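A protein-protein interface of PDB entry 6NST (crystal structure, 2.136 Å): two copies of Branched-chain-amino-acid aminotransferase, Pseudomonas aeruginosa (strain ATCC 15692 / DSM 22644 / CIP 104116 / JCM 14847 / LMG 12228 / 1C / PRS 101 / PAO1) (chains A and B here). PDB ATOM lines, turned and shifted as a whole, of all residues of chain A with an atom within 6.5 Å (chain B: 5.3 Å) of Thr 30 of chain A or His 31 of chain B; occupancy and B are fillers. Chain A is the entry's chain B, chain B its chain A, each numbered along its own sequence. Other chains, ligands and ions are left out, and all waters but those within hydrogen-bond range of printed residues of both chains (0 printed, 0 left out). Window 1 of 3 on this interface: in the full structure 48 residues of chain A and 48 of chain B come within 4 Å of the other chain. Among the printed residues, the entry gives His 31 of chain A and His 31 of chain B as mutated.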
ATOM      1  N   THR A  24       8.025  14.276  26.037  1.00  0.00           N
ATOM      2  CA  THR A  24       8.405  15.125  27.153  1.00  0.00           C
ATOM      3  C   THR A  24       7.141  15.727  27.742  1.00  0.00           C
ATOM      4  O   THR A  24       6.117  15.846  27.064  1.00  0.00           O
ATOM      5  CB  THR A  24       9.383  16.228  26.730  1.00  0.00           C
ATOM      6  OG1 THR A  24       9.717  17.032  27.868  1.00  0.00           O
ATOM      7  CG2 THR A  24       8.768  17.109  25.653  1.00  0.00           C
ATOM      8  N   HIS A  25       7.221  16.099  29.016  1.00  0.00           N
ATOM      9  CA  HIS A  25       6.059  16.645  29.701  1.00  0.00           C
ATOM     10  C   HIS A  25       5.639  17.964  29.064  1.00  0.00           C
ATOM     11  O   HIS A  25       6.459  18.712  28.526  1.00  0.00           O
ATOM     12  CB  HIS A  25       6.355  16.847  31.187  1.00  0.00           C
ATOM     13  CG  HIS A  25       5.131  17.072  32.019  1.00  0.00           C
ATOM     14  ND1 HIS A  25       4.676  18.331  32.350  1.00  0.00           N
ATOM     15  CD2 HIS A  25       4.263  16.199  32.583  1.00  0.00           C
ATOM     16  CE1 HIS A  25       3.583  18.223  33.083  1.00  0.00           C
ATOM     17  NE2 HIS A  25       3.310  16.939  33.238  1.00  0.00           N
ATOM     18  N   LEU A  27       4.627  20.616  30.452  1.00  0.00           N
ATOM     19  CA  LEU A  27       5.174  21.759  31.174  1.00  0.00           C
ATOM     20  C   LEU A  27       6.680  21.887  30.995  1.00  0.00           C
ATOM     21  O   LEU A  27       7.366  22.428  31.873  1.00  0.00           O
ATOM     22  CB  LEU A  27       4.808  21.671  32.655  1.00  0.00           C
ATOM     23  CG  LEU A  27       3.305  21.712  32.930  1.00  0.00           C
ATOM     24  CD1 LEU A  27       3.019  21.735  34.422  1.00  0.00           C
ATOM     25  CD2 LEU A  27       2.671  22.909  32.239  1.00  0.00           C
ATOM     26  N   THR A  28       7.209  21.393  29.879  1.00  0.00           N
ATOM     27  CA  THR A  28       8.627  21.531  29.586  1.00  0.00           C
ATOM     28  C   THR A  28       8.987  23.004  29.440  1.00  0.00           C
ATOM     29  O   THR A  28       8.280  23.771  28.782  1.00  0.00           O
ATOM     30  CB  THR A  28       8.972  20.763  28.310  1.00  0.00           C
ATOM     31  OG1 THR A  28       8.589  19.389  28.461  1.00  0.00           O
ATOM     32  CG2 THR A  28      10.454  20.826  28.031  1.00  0.00           C
ATOM     33  N   HIS A  29      10.100  23.395  30.068  1.00  0.00           N
ATOM     34  CA  HIS A  29      10.448  24.811  30.159  1.00  0.00           C
ATOM     35  C   HIS A  29      10.682  25.419  28.780  1.00  0.00           C
ATOM     36  O   HIS A  29      10.146  26.488  28.462  1.00  0.00           O
ATOM     37  CB  HIS A  29      11.680  24.986  31.047  1.00  0.00           C
ATOM     38  CG  HIS A  29      11.844  26.374  31.584  1.00  0.00           C
ATOM     39  ND1 HIS A  29      12.661  27.311  30.989  1.00  0.00           N
ATOM     40  CD2 HIS A  29      11.296  26.982  32.662  1.00  0.00           C
ATOM     41  CE1 HIS A  29      12.609  28.437  31.678  1.00  0.00           C
ATOM     42  NE2 HIS A  29      11.787  28.265  32.697  1.00  0.00           N
ATOM     43  N   THR A  30      11.486  24.751  27.943  1.00  0.00           N
ATOM     44  CA  THR A  30      11.768  25.272  26.608  1.00  0.00           C
ATOM     45  C   THR A  30      10.495  25.407  25.783  1.00  0.00           C
ATOM     46  O   THR A  30      10.377  26.327  24.965  1.00  0.00           O
ATOM     47  CB  THR A  30      12.774  24.366  25.894  1.00  0.00           C
ATOM     48  OG1 THR A  30      14.017  24.373  26.608  1.00  0.00           O
ATOM     49  CG2 THR A  30      13.015  24.830  24.463  1.00  0.00           C
ATOM     50  N   HIS A  31       9.530  24.513  25.993  1.00  0.00           N
ATOM     51  CA  HIS A  31       8.263  24.595  25.277  1.00  0.00           C
ATOM     52  C   HIS A  31       7.539  25.900  25.580  1.00  0.00           C
ATOM     53  O   HIS A  31       6.915  26.486  24.689  1.00  0.00           O
ATOM     54  CB  HIS A  31       7.392  23.396  25.652  1.00  0.00           C
ATOM     55  CG  HIS A  31       6.345  23.062  24.639  1.00  0.00           C
ATOM     56  ND1 HIS A  31       5.615  21.894  24.684  1.00  0.00           N
ATOM     57  CD2 HIS A  31       5.907  23.740  23.553  1.00  0.00           C
ATOM     58  CE1 HIS A  31       4.771  21.867  23.669  1.00  0.00           C
ATOM     59  NE2 HIS A  31       4.927  22.974  22.967  1.00  0.00           N
ATOM     60  N   HIS A  32       7.637  26.384  26.818  1.00  0.00           N
ATOM     61  CA  HIS A  32       6.867  27.539  27.256  1.00  0.00           C
ATOM     62  C   HIS A  32       7.604  28.861  27.098  1.00  0.00           C
ATOM     63  O   HIS A  32       6.957  29.904  26.963  1.00  0.00           O
ATOM     64  CB  HIS A  32       6.462  27.376  28.723  1.00  0.00           C
ATOM     65  CG  HIS A  32       5.389  26.357  28.949  1.00  0.00           C
ATOM     66  ND1 HIS A  32       4.102  26.698  29.305  1.00  0.00           N
ATOM     67  CD2 HIS A  32       5.412  25.005  28.875  1.00  0.00           C
ATOM     68  CE1 HIS A  32       3.377  25.602  29.435  1.00  0.00           C
ATOM     69  NE2 HIS A  32       4.149  24.560  29.183  1.00  0.00           N
ATOM     70  N   TYR A  33       8.937  28.856  27.122  1.00  0.00           N
ATOM     71  CA  TYR A  33       9.700  30.095  27.123  1.00  0.00           C
ATOM     72  C   TYR A  33      10.708  30.200  25.988  1.00  0.00           C
ATOM     73  O   TYR A  33      11.372  31.237  25.868  1.00  0.00           O
ATOM     74  CB  TYR A  33      10.413  30.270  28.471  1.00  0.00           C
ATOM     75  CG  TYR A  33       9.461  30.268  29.647  1.00  0.00           C
ATOM     76  CD1 TYR A  33       8.530  31.288  29.811  1.00  0.00           C
ATOM     77  CD2 TYR A  33       9.486  29.243  30.585  1.00  0.00           C
ATOM     78  CE1 TYR A  33       7.651  31.290  30.880  1.00  0.00           C
ATOM     79  CE2 TYR A  33       8.611  29.237  31.659  1.00  0.00           C
ATOM     80  CZ  TYR A  33       7.697  30.262  31.799  1.00  0.00           C
ATOM     81  OH  TYR A  33       6.826  30.259  32.864  1.00  0.00           O
ATOM     82  N   GLY A  34      10.843  29.171  25.154  1.00  0.00           N
ATOM     83  CA  GLY A  34      11.676  29.244  23.971  1.00  0.00           C
ATOM     84  C   GLY A  34      13.162  29.081  24.200  1.00  0.00           C
ATOM     85  O   GLY A  34      13.918  29.049  23.221  1.00  0.00           O
ATOM     86  N   MET A  35      13.607  28.970  25.449  1.00  0.00           N
ATOM     87  CA  MET A  35      15.029  28.833  25.764  1.00  0.00           C
ATOM     88  C   MET A  35      15.502  27.447  25.346  1.00  0.00           C
ATOM     89  O   MET A  35      15.339  26.469  26.080  1.00  0.00           O
ATOM     90  CB  MET A  35      15.267  29.075  27.249  1.00  0.00           C
ATOM     91  CG  MET A  35      16.725  29.013  27.680  1.00  0.00           C
ATOM     92  SD  MET A  35      17.737  30.304  26.934  1.00  0.00           S
ATOM     93  CE  MET A  35      18.723  30.814  28.338  1.00  0.00           C
ATOM     94  N   GLY A  36      16.091  27.362  24.164  1.00  0.00           N
ATOM     95  CA  GLY A  36      16.628  26.109  23.676  1.00  0.00           C
ATOM     96  C   GLY A  36      17.359  26.353  22.375  1.00  0.00           C
ATOM     97  O   GLY A  36      17.138  27.358  21.692  1.00  0.00           O
ATOM     98  N   VAL A  37      18.246  25.415  22.048  1.00  0.00           N
ATOM     99  CA  VAL A  37      19.050  25.507  20.837  1.00  0.00           C
ATOM    100  C   VAL A  37      18.917  24.209  20.054  1.00  0.00           C
ATOM    101  O   VAL A  37      18.734  23.128  20.626  1.00  0.00           O
ATOM    102  CB  VAL A  37      20.532  25.820  21.149  1.00  0.00           C
ATOM    103  CG1 VAL A  37      20.640  27.106  21.964  1.00  0.00           C
ATOM    104  CG2 VAL A  37      21.190  24.663  21.886  1.00  0.00           C
ATOM    105  N   MET A  71      23.608  27.187  28.655  1.00  0.00           N
ATOM    106  CA  MET A  71      23.097  25.829  28.785  1.00  0.00           C
ATOM    107  C   MET A  71      24.256  24.847  28.697  1.00  0.00           C
ATOM    108  O   MET A  71      25.038  24.884  27.739  1.00  0.00           O
ATOM    109  CB  MET A  71      22.060  25.525  27.702  1.00  0.00           C
ATOM    110  CG  MET A  71      20.833  26.421  27.742  1.00  0.00           C
ATOM    111  SD  MET A  71      19.634  26.025  26.454  1.00  0.00           S
ATOM    112  CE  MET A  71      19.165  24.363  26.924  1.00  0.00           C
ATOM    113  N   MET A 101      18.575  18.705  19.087  1.00  0.00           N
ATOM    114  CA  MET A 101      17.890  19.753  19.831  1.00  0.00           C
ATOM    115  C   MET A 101      18.240  19.657  21.307  1.00  0.00           C
ATOM    116  O   MET A 101      18.105  18.590  21.915  1.00  0.00           O
ATOM    117  CB  MET A 101      16.372  19.661  19.628  1.00  0.00           C
ATOM    118  CG  MET A 101      15.632  20.969  19.861  1.00  0.00           C
ATOM    119  SD  MET A 101      14.934  21.113  21.515  1.00  0.00           S
ATOM    120  CE  MET A 101      13.599  19.921  21.421  1.00  0.00           C
ATOM    121  N   VAL A 102      18.691  20.775  21.872  1.00  0.00           N
ATOM    122  CA  VAL A 102      19.047  20.882  23.283  1.00  0.00           C
ATOM    123  C   VAL A 102      18.028  21.789  23.956  1.00  0.00           C
ATOM    124  O   VAL A 102      17.818  22.926  23.517  1.00  0.00           O
ATOM    125  CB  VAL A 102      20.472  21.433  23.464  1.00  0.00           C
ATOM    126  CG1 VAL A 102      20.784  21.619  24.936  1.00  0.00           C
ATOM    127  CG2 VAL A 102      21.488  20.510  22.804  1.00  0.00           C
ATOM    128  N   PHE A 103      17.400  21.295  25.022  1.00  0.00           N
ATOM    129  CA  PHE A 103      16.321  22.041  25.648  1.00  0.00           C
ATOM    130  C   PHE A 103      16.326  21.816  27.153  1.00  0.00           C
ATOM    131  O   PHE A 103      16.931  20.869  27.663  1.00  0.00           O
ATOM    132  CB  PHE A 103      14.958  21.657  25.054  1.00  0.00           C
ATOM    133  CG  PHE A 103      14.553  20.231  25.314  1.00  0.00           C
ATOM    134  CD1 PHE A 103      13.659  19.926  26.330  1.00  0.00           C
ATOM    135  CD2 PHE A 103      15.048  19.198  24.535  1.00  0.00           C
ATOM    136  CE1 PHE A 103      13.275  18.620  26.569  1.00  0.00           C
ATOM    137  CE2 PHE A 103      14.668  17.890  24.769  1.00  0.00           C
ATOM    138  CZ  PHE A 103      13.780  17.600  25.787  1.00  0.00           C
ATOM    139  N   TYR A 104      15.643  22.718  27.855  1.00  0.00           N
ATOM    140  CA  TYR A 104      15.447  22.593  29.291  1.00  0.00           C
ATOM    141  C   TYR A 104      14.230  21.723  29.574  1.00  0.00           C
ATOM    142  O   TYR A 104      13.200  21.841  28.908  1.00  0.00           O
ATOM    143  CB  TYR A 104      15.257  23.971  29.927  1.00  0.00           C
ATOM    144  CG  TYR A 104      16.533  24.725  30.226  1.00  0.00           C
ATOM    145  CD1 TYR A 104      17.650  24.074  30.733  1.00  0.00           C
ATOM    146  CD2 TYR A 104      16.615  26.097  30.013  1.00  0.00           C
ATOM    147  CE1 TYR A 104      18.814  24.769  31.018  1.00  0.00           C
ATOM    148  CE2 TYR A 104      17.774  26.799  30.290  1.00  0.00           C
ATOM    149  CZ  TYR A 104      18.870  26.131  30.792  1.00  0.00           C
ATOM    150  OH  TYR A 104      20.023  26.827  31.069  1.00  0.00           O
ATOM    151  N   GLY A 105      14.353  20.851  30.571  1.00  0.00           N
ATOM    152  CA  GLY A 105      13.290  19.934  30.916  1.00  0.00           C
ATOM    153  C   GLY A 105      12.190  20.592  31.729  1.00  0.00           C
ATOM    154  O   GLY A 105      12.135  21.811  31.907  1.00  0.00           O
ATOM    155  N   ASN A 162      15.595  28.276  19.660  1.00  0.00           N
ATOM    156  CA  ASN A 162      14.261  27.805  19.297  1.00  0.00           C
ATOM    157  C   ASN A 162      13.269  28.958  19.203  1.00  0.00           C
ATOM    158  O   ASN A 162      12.616  29.152  18.172  1.00  0.00           O
ATOM    159  CB  ASN A 162      13.775  26.769  20.316  1.00  0.00           C
ATOM    160  CG  ASN A 162      14.649  25.531  20.356  1.00  0.00           C
ATOM    161  OD1 ASN A 162      15.761  25.522  19.829  1.00  0.00           O
ATOM    162  ND2 ASN A 162      14.149  24.475  20.987  1.00  0.00           N
ATOM    163  N   GLY A 163      13.136  29.733  20.281  1.00  0.00           N
ATOM    164  CA  GLY A 163      12.134  30.782  20.331  1.00  0.00           C
ATOM    165  C   GLY A 163      12.358  31.911  19.349  1.00  0.00           C
ATOM    166  O   GLY A 163      11.417  32.657  19.056  1.00  0.00           O
ATOM    167  N   HIS B  25       5.035  14.970  22.216  1.00  0.00           N
ATOM    168  CA  HIS B  25       6.181  14.410  21.520  1.00  0.00           C
ATOM    169  C   HIS B  25       7.329  15.411  21.525  1.00  0.00           C
ATOM    170  O   HIS B  25       7.123  16.627  21.506  1.00  0.00           O
ATOM    171  CB  HIS B  25       5.815  14.028  20.089  1.00  0.00           C
ATOM    172  CG  HIS B  25       6.842  13.173  19.415  1.00  0.00           C
ATOM    173  ND1 HIS B  25       7.708  13.661  18.461  1.00  0.00           N
ATOM    174  CD2 HIS B  25       7.147  11.862  19.566  1.00  0.00           C
ATOM    175  CE1 HIS B  25       8.499  12.687  18.048  1.00  0.00           C
ATOM    176  NE2 HIS B  25       8.179  11.585  18.702  1.00  0.00           N
ATOM    177  N   VAL B  26       8.554  14.886  21.568  1.00  0.00           N
ATOM    178  CA  VAL B  26       9.723  15.752  21.652  1.00  0.00           C
ATOM    179  C   VAL B  26       9.961  16.534  20.371  1.00  0.00           C
ATOM    180  O   VAL B  26      10.727  17.505  20.381  1.00  0.00           O
ATOM    181  CB  VAL B  26      10.968  14.926  22.036  1.00  0.00           C
ATOM    182  CG1 VAL B  26      11.654  14.365  20.795  1.00  0.00           C
ATOM    183  CG2 VAL B  26      11.918  15.767  22.870  1.00  0.00           C
ATOM    184  N   THR B  28       7.602  18.317  19.047  1.00  0.00           N
ATOM    185  CA  THR B  28       6.538  19.312  19.037  1.00  0.00           C
ATOM    186  C   THR B  28       7.029  20.602  18.388  1.00  0.00           C
ATOM    187  O   THR B  28       8.149  21.055  18.637  1.00  0.00           O
ATOM    188  CB  THR B  28       6.064  19.576  20.468  1.00  0.00           C
ATOM    189  OG1 THR B  28       5.673  18.339  21.078  1.00  0.00           O
ATOM    190  CG2 THR B  28       4.887  20.521  20.478  1.00  0.00           C
ATOM    191  N   HIS B  29       6.176  21.196  17.546  1.00  0.00           N
ATOM    192  CA  HIS B  29       6.597  22.332  16.729  1.00  0.00           C
ATOM    193  C   HIS B  29       6.911  23.555  17.586  1.00  0.00           C
ATOM    194  O   HIS B  29       7.948  24.205  17.401  1.00  0.00           O
ATOM    195  CB  HIS B  29       5.518  22.657  15.696  1.00  0.00           C
ATOM    196  CG  HIS B  29       5.976  23.582  14.612  1.00  0.00           C
ATOM    197  ND1 HIS B  29       5.977  24.953  14.752  1.00  0.00           N
ATOM    198  CD2 HIS B  29       6.439  23.332  13.363  1.00  0.00           C
ATOM    199  CE1 HIS B  29       6.421  25.508  13.639  1.00  0.00           C
ATOM    200  NE2 HIS B  29       6.709  24.546  12.780  1.00  0.00           N
ATOM    201  N   THR B  30       6.024  23.892  18.527  1.00  0.00           N
ATOM    202  CA  THR B  30       6.298  25.010  19.426  1.00  0.00           C
ATOM    203  C   THR B  30       7.554  24.762  20.254  1.00  0.00           C
ATOM    204  O   THR B  30       8.272  25.709  20.596  1.00  0.00           O
ATOM    205  CB  THR B  30       5.093  25.263  20.336  1.00  0.00           C
ATOM    206  OG1 THR B  30       3.940  25.547  19.534  1.00  0.00           O
ATOM    207  CG2 THR B  30       5.347  26.444  21.271  1.00  0.00           C
ATOM    208  N   HIS B  31       7.844  23.496  20.564  1.00  0.00           N
ATOM    209  CA  HIS B  31       9.047  23.165  21.319  1.00  0.00           C
ATOM    210  C   HIS B  31      10.312  23.552  20.561  1.00  0.00           C
ATOM    211  O   HIS B  31      11.322  23.910  21.178  1.00  0.00           O
ATOM    212  CB  HIS B  31       9.062  21.669  21.636  1.00  0.00           C
ATOM    213  CG  HIS B  31       9.827  21.314  22.872  1.00  0.00           C
ATOM    214  ND1 HIS B  31      10.218  20.023  23.160  1.00  0.00           N
ATOM    215  CD2 HIS B  31      10.259  22.077  23.903  1.00  0.00           C
ATOM    216  CE1 HIS B  31      10.865  20.009  24.311  1.00  0.00           C
ATOM    217  NE2 HIS B  31      10.902  21.242  24.783  1.00  0.00           N
ATOM    218  N   HIS B  32      10.274  23.492  19.229  1.00  0.00           N
ATOM    219  CA  HIS B  32      11.450  23.750  18.410  1.00  0.00           C
ATOM    220  C   HIS B  32      11.494  25.157  17.833  1.00  0.00           C
ATOM    221  O   HIS B  32      12.584  25.636  17.503  1.00  0.00           O
ATOM    222  CB  HIS B  32      11.529  22.741  17.256  1.00  0.00           C
ATOM    223  CG  HIS B  32      11.847  21.346  17.692  1.00  0.00           C
ATOM    224  ND1 HIS B  32      13.058  20.744  17.431  1.00  0.00           N
ATOM    225  CD2 HIS B  32      11.111  20.434  18.372  1.00  0.00           C
ATOM    226  CE1 HIS B  32      13.056  19.520  17.930  1.00  0.00           C
ATOM    227  NE2 HIS B  32      11.886  19.308  18.507  1.00  0.00           N
ATOM    228  N   TYR B  33      10.350  25.827  17.701  1.00  0.00           N
ATOM    229  CA  TYR B  33      10.307  27.133  17.062  1.00  0.00           C
ATOM    230  C   TYR B  33       9.639  28.211  17.905  1.00  0.00           C
ATOM    231  O   TYR B  33       9.545  29.356  17.446  1.00  0.00           O
ATOM    232  CB  TYR B  33       9.602  27.033  15.702  1.00  0.00           C
ATOM    233  CG  TYR B  33      10.246  26.028  14.773  1.00  0.00           C
ATOM    234  CD1 TYR B  33      11.422  26.334  14.098  1.00  0.00           C
ATOM    235  CD2 TYR B  33       9.684  24.773  14.575  1.00  0.00           C
ATOM    236  CE1 TYR B  33      12.017  25.422  13.250  1.00  0.00           C
ATOM    237  CE2 TYR B  33      10.272  23.852  13.727  1.00  0.00           C
ATOM    238  CZ  TYR B  33      11.439  24.182  13.068  1.00  0.00           C
ATOM    239  OH  TYR B  33      12.031  23.271  12.223  1.00  0.00           O
ATOM    240  N   GLY B  34       9.177  27.888  19.111  1.00  0.00           N
ATOM    241  CA  GLY B  34       8.648  28.884  20.022  1.00  0.00           C
ATOM    242  C   GLY B  34       7.307  29.476  19.650  1.00  0.00           C
ATOM    243  O   GLY B  34       6.786  30.299  20.411  1.00  0.00           O
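The backbone carbonyl oxygen (O) of His 31 of chain B is in hydrogen-bond range of the side-chain amide nitrogen (ND2) of Asn 162 of chain A, at 2.9 Å.
The backbone carbonyl oxygen (O) of Asn 162 of chain A sits close to the backbone carbonyl oxygen (O) of Tyr 33 of chain B (3.2 Å).
The backbone carbonyl oxygen of Gly 34 of chain A is in hydrogen-bond range of the backbone NH of Gly 163 of chain A, at 3.1 Å.
O of Val 26 of chain B is in hydrogen-bond range of NE2 of His 32 of chain B, at 2.8 Å.
The side-chain sulfur of Met 101 of chain A is in hydrogen-bond range of the side-chain amide nitrogen of Asn 162 of chain A.
The backbone NH of Tyr 104 of chain A sits at hydrogen-bond distance from the side-chain hydroxyl of Thr 30 of chain A (2.6 Å).
OD1 of Asn 162 of chain A lies within hydrogen-bond range of N of Val 37 of chain A (3.3 Å).
O of Met 35 of chain A lies within hydrogen-bond range of OG1 of Thr 30 of chain A, 2.5 Å away.
CE1 of His 31 of chain B touches CG2 of Thr 24 of chain A, at 3.8 Å.
Thr 30 of chain A touches His 31 of chain B (CB to NE2, 3.8 Å).
Thr 30 of chain B touches His 31 of chain A.
His 31 of chain B touches His 31 of chain A (CD2 to N, 3.3 Å).
CE of Met 101 of chain A touches O of Val 26 of chain B, at 3.9 Å.
CE of Met 101 of chain A touches ND1 of His 31 of chain B, 3.8 Å away.
His 32 of chain B touches Met 101 of chain A (NE2 to CE, 3.4 Å).
CD1 of Phe 103 of chain A touches NE2 of His 31 of chain B (3.4 Å).
His 32 of chain B touches Asn 162 of chain A.
Gly 163 of chain A touches Gly 34 of chain B (CA to CA, 3.98 Å).
His 25 of chain A touches none of the printed residues of chain B.
Thr 30 of chain A touches just one residue of chain B: His 31.
Of the printed residues of chain B, His 31 of chain A touches Thr 28 (3.5 Å), Thr 30 (3.5 Å) and His 31 (3.3 Å).
Met 35 of chain A touches none of the printed residues of chain B.
Of the printed residues of chain A, Gly 34 of chain B touches Asn 162 (3.8 Å) and Gly 163 (3.98 Å).
The nearest residue of chain B that does not touch Thr 30 of chain A is Thr 30 of chain B (4.9 Å).
Of the 9 printed residues of chain B, 7 touch a printed residue of chain A.
Hydrophobic or aromatic side chains of chain B that line the printed part of chain A: Val 26, His 31 and His 32.
Of the 21 printed residues of chain A, 8 touch a printed residue of chain B.
Hydrophobic or aromatic side chains of chain A within 4 Å of the printed part of chain B: His 31, Met 101 and Phe 103.
Among the printed residues, 16 pairs touch across the chains.
Among the printed residues, no Asp or Glu carboxylate lies within 4 Å of a Lys or Arg side-chain nitrogen of the other chain.
Thr 28 of chain A touches His 31 of chain B, and with the chains exchanged His 31 of chain A touches Thr 28 of chain B.
Thr 30 of chain A touches His 31 of chain B, and with the chains exchanged His 31 of chain A touches Thr 30 of chain B.
His 31 of chain A touches its own counterpart, His 31 of chain B.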
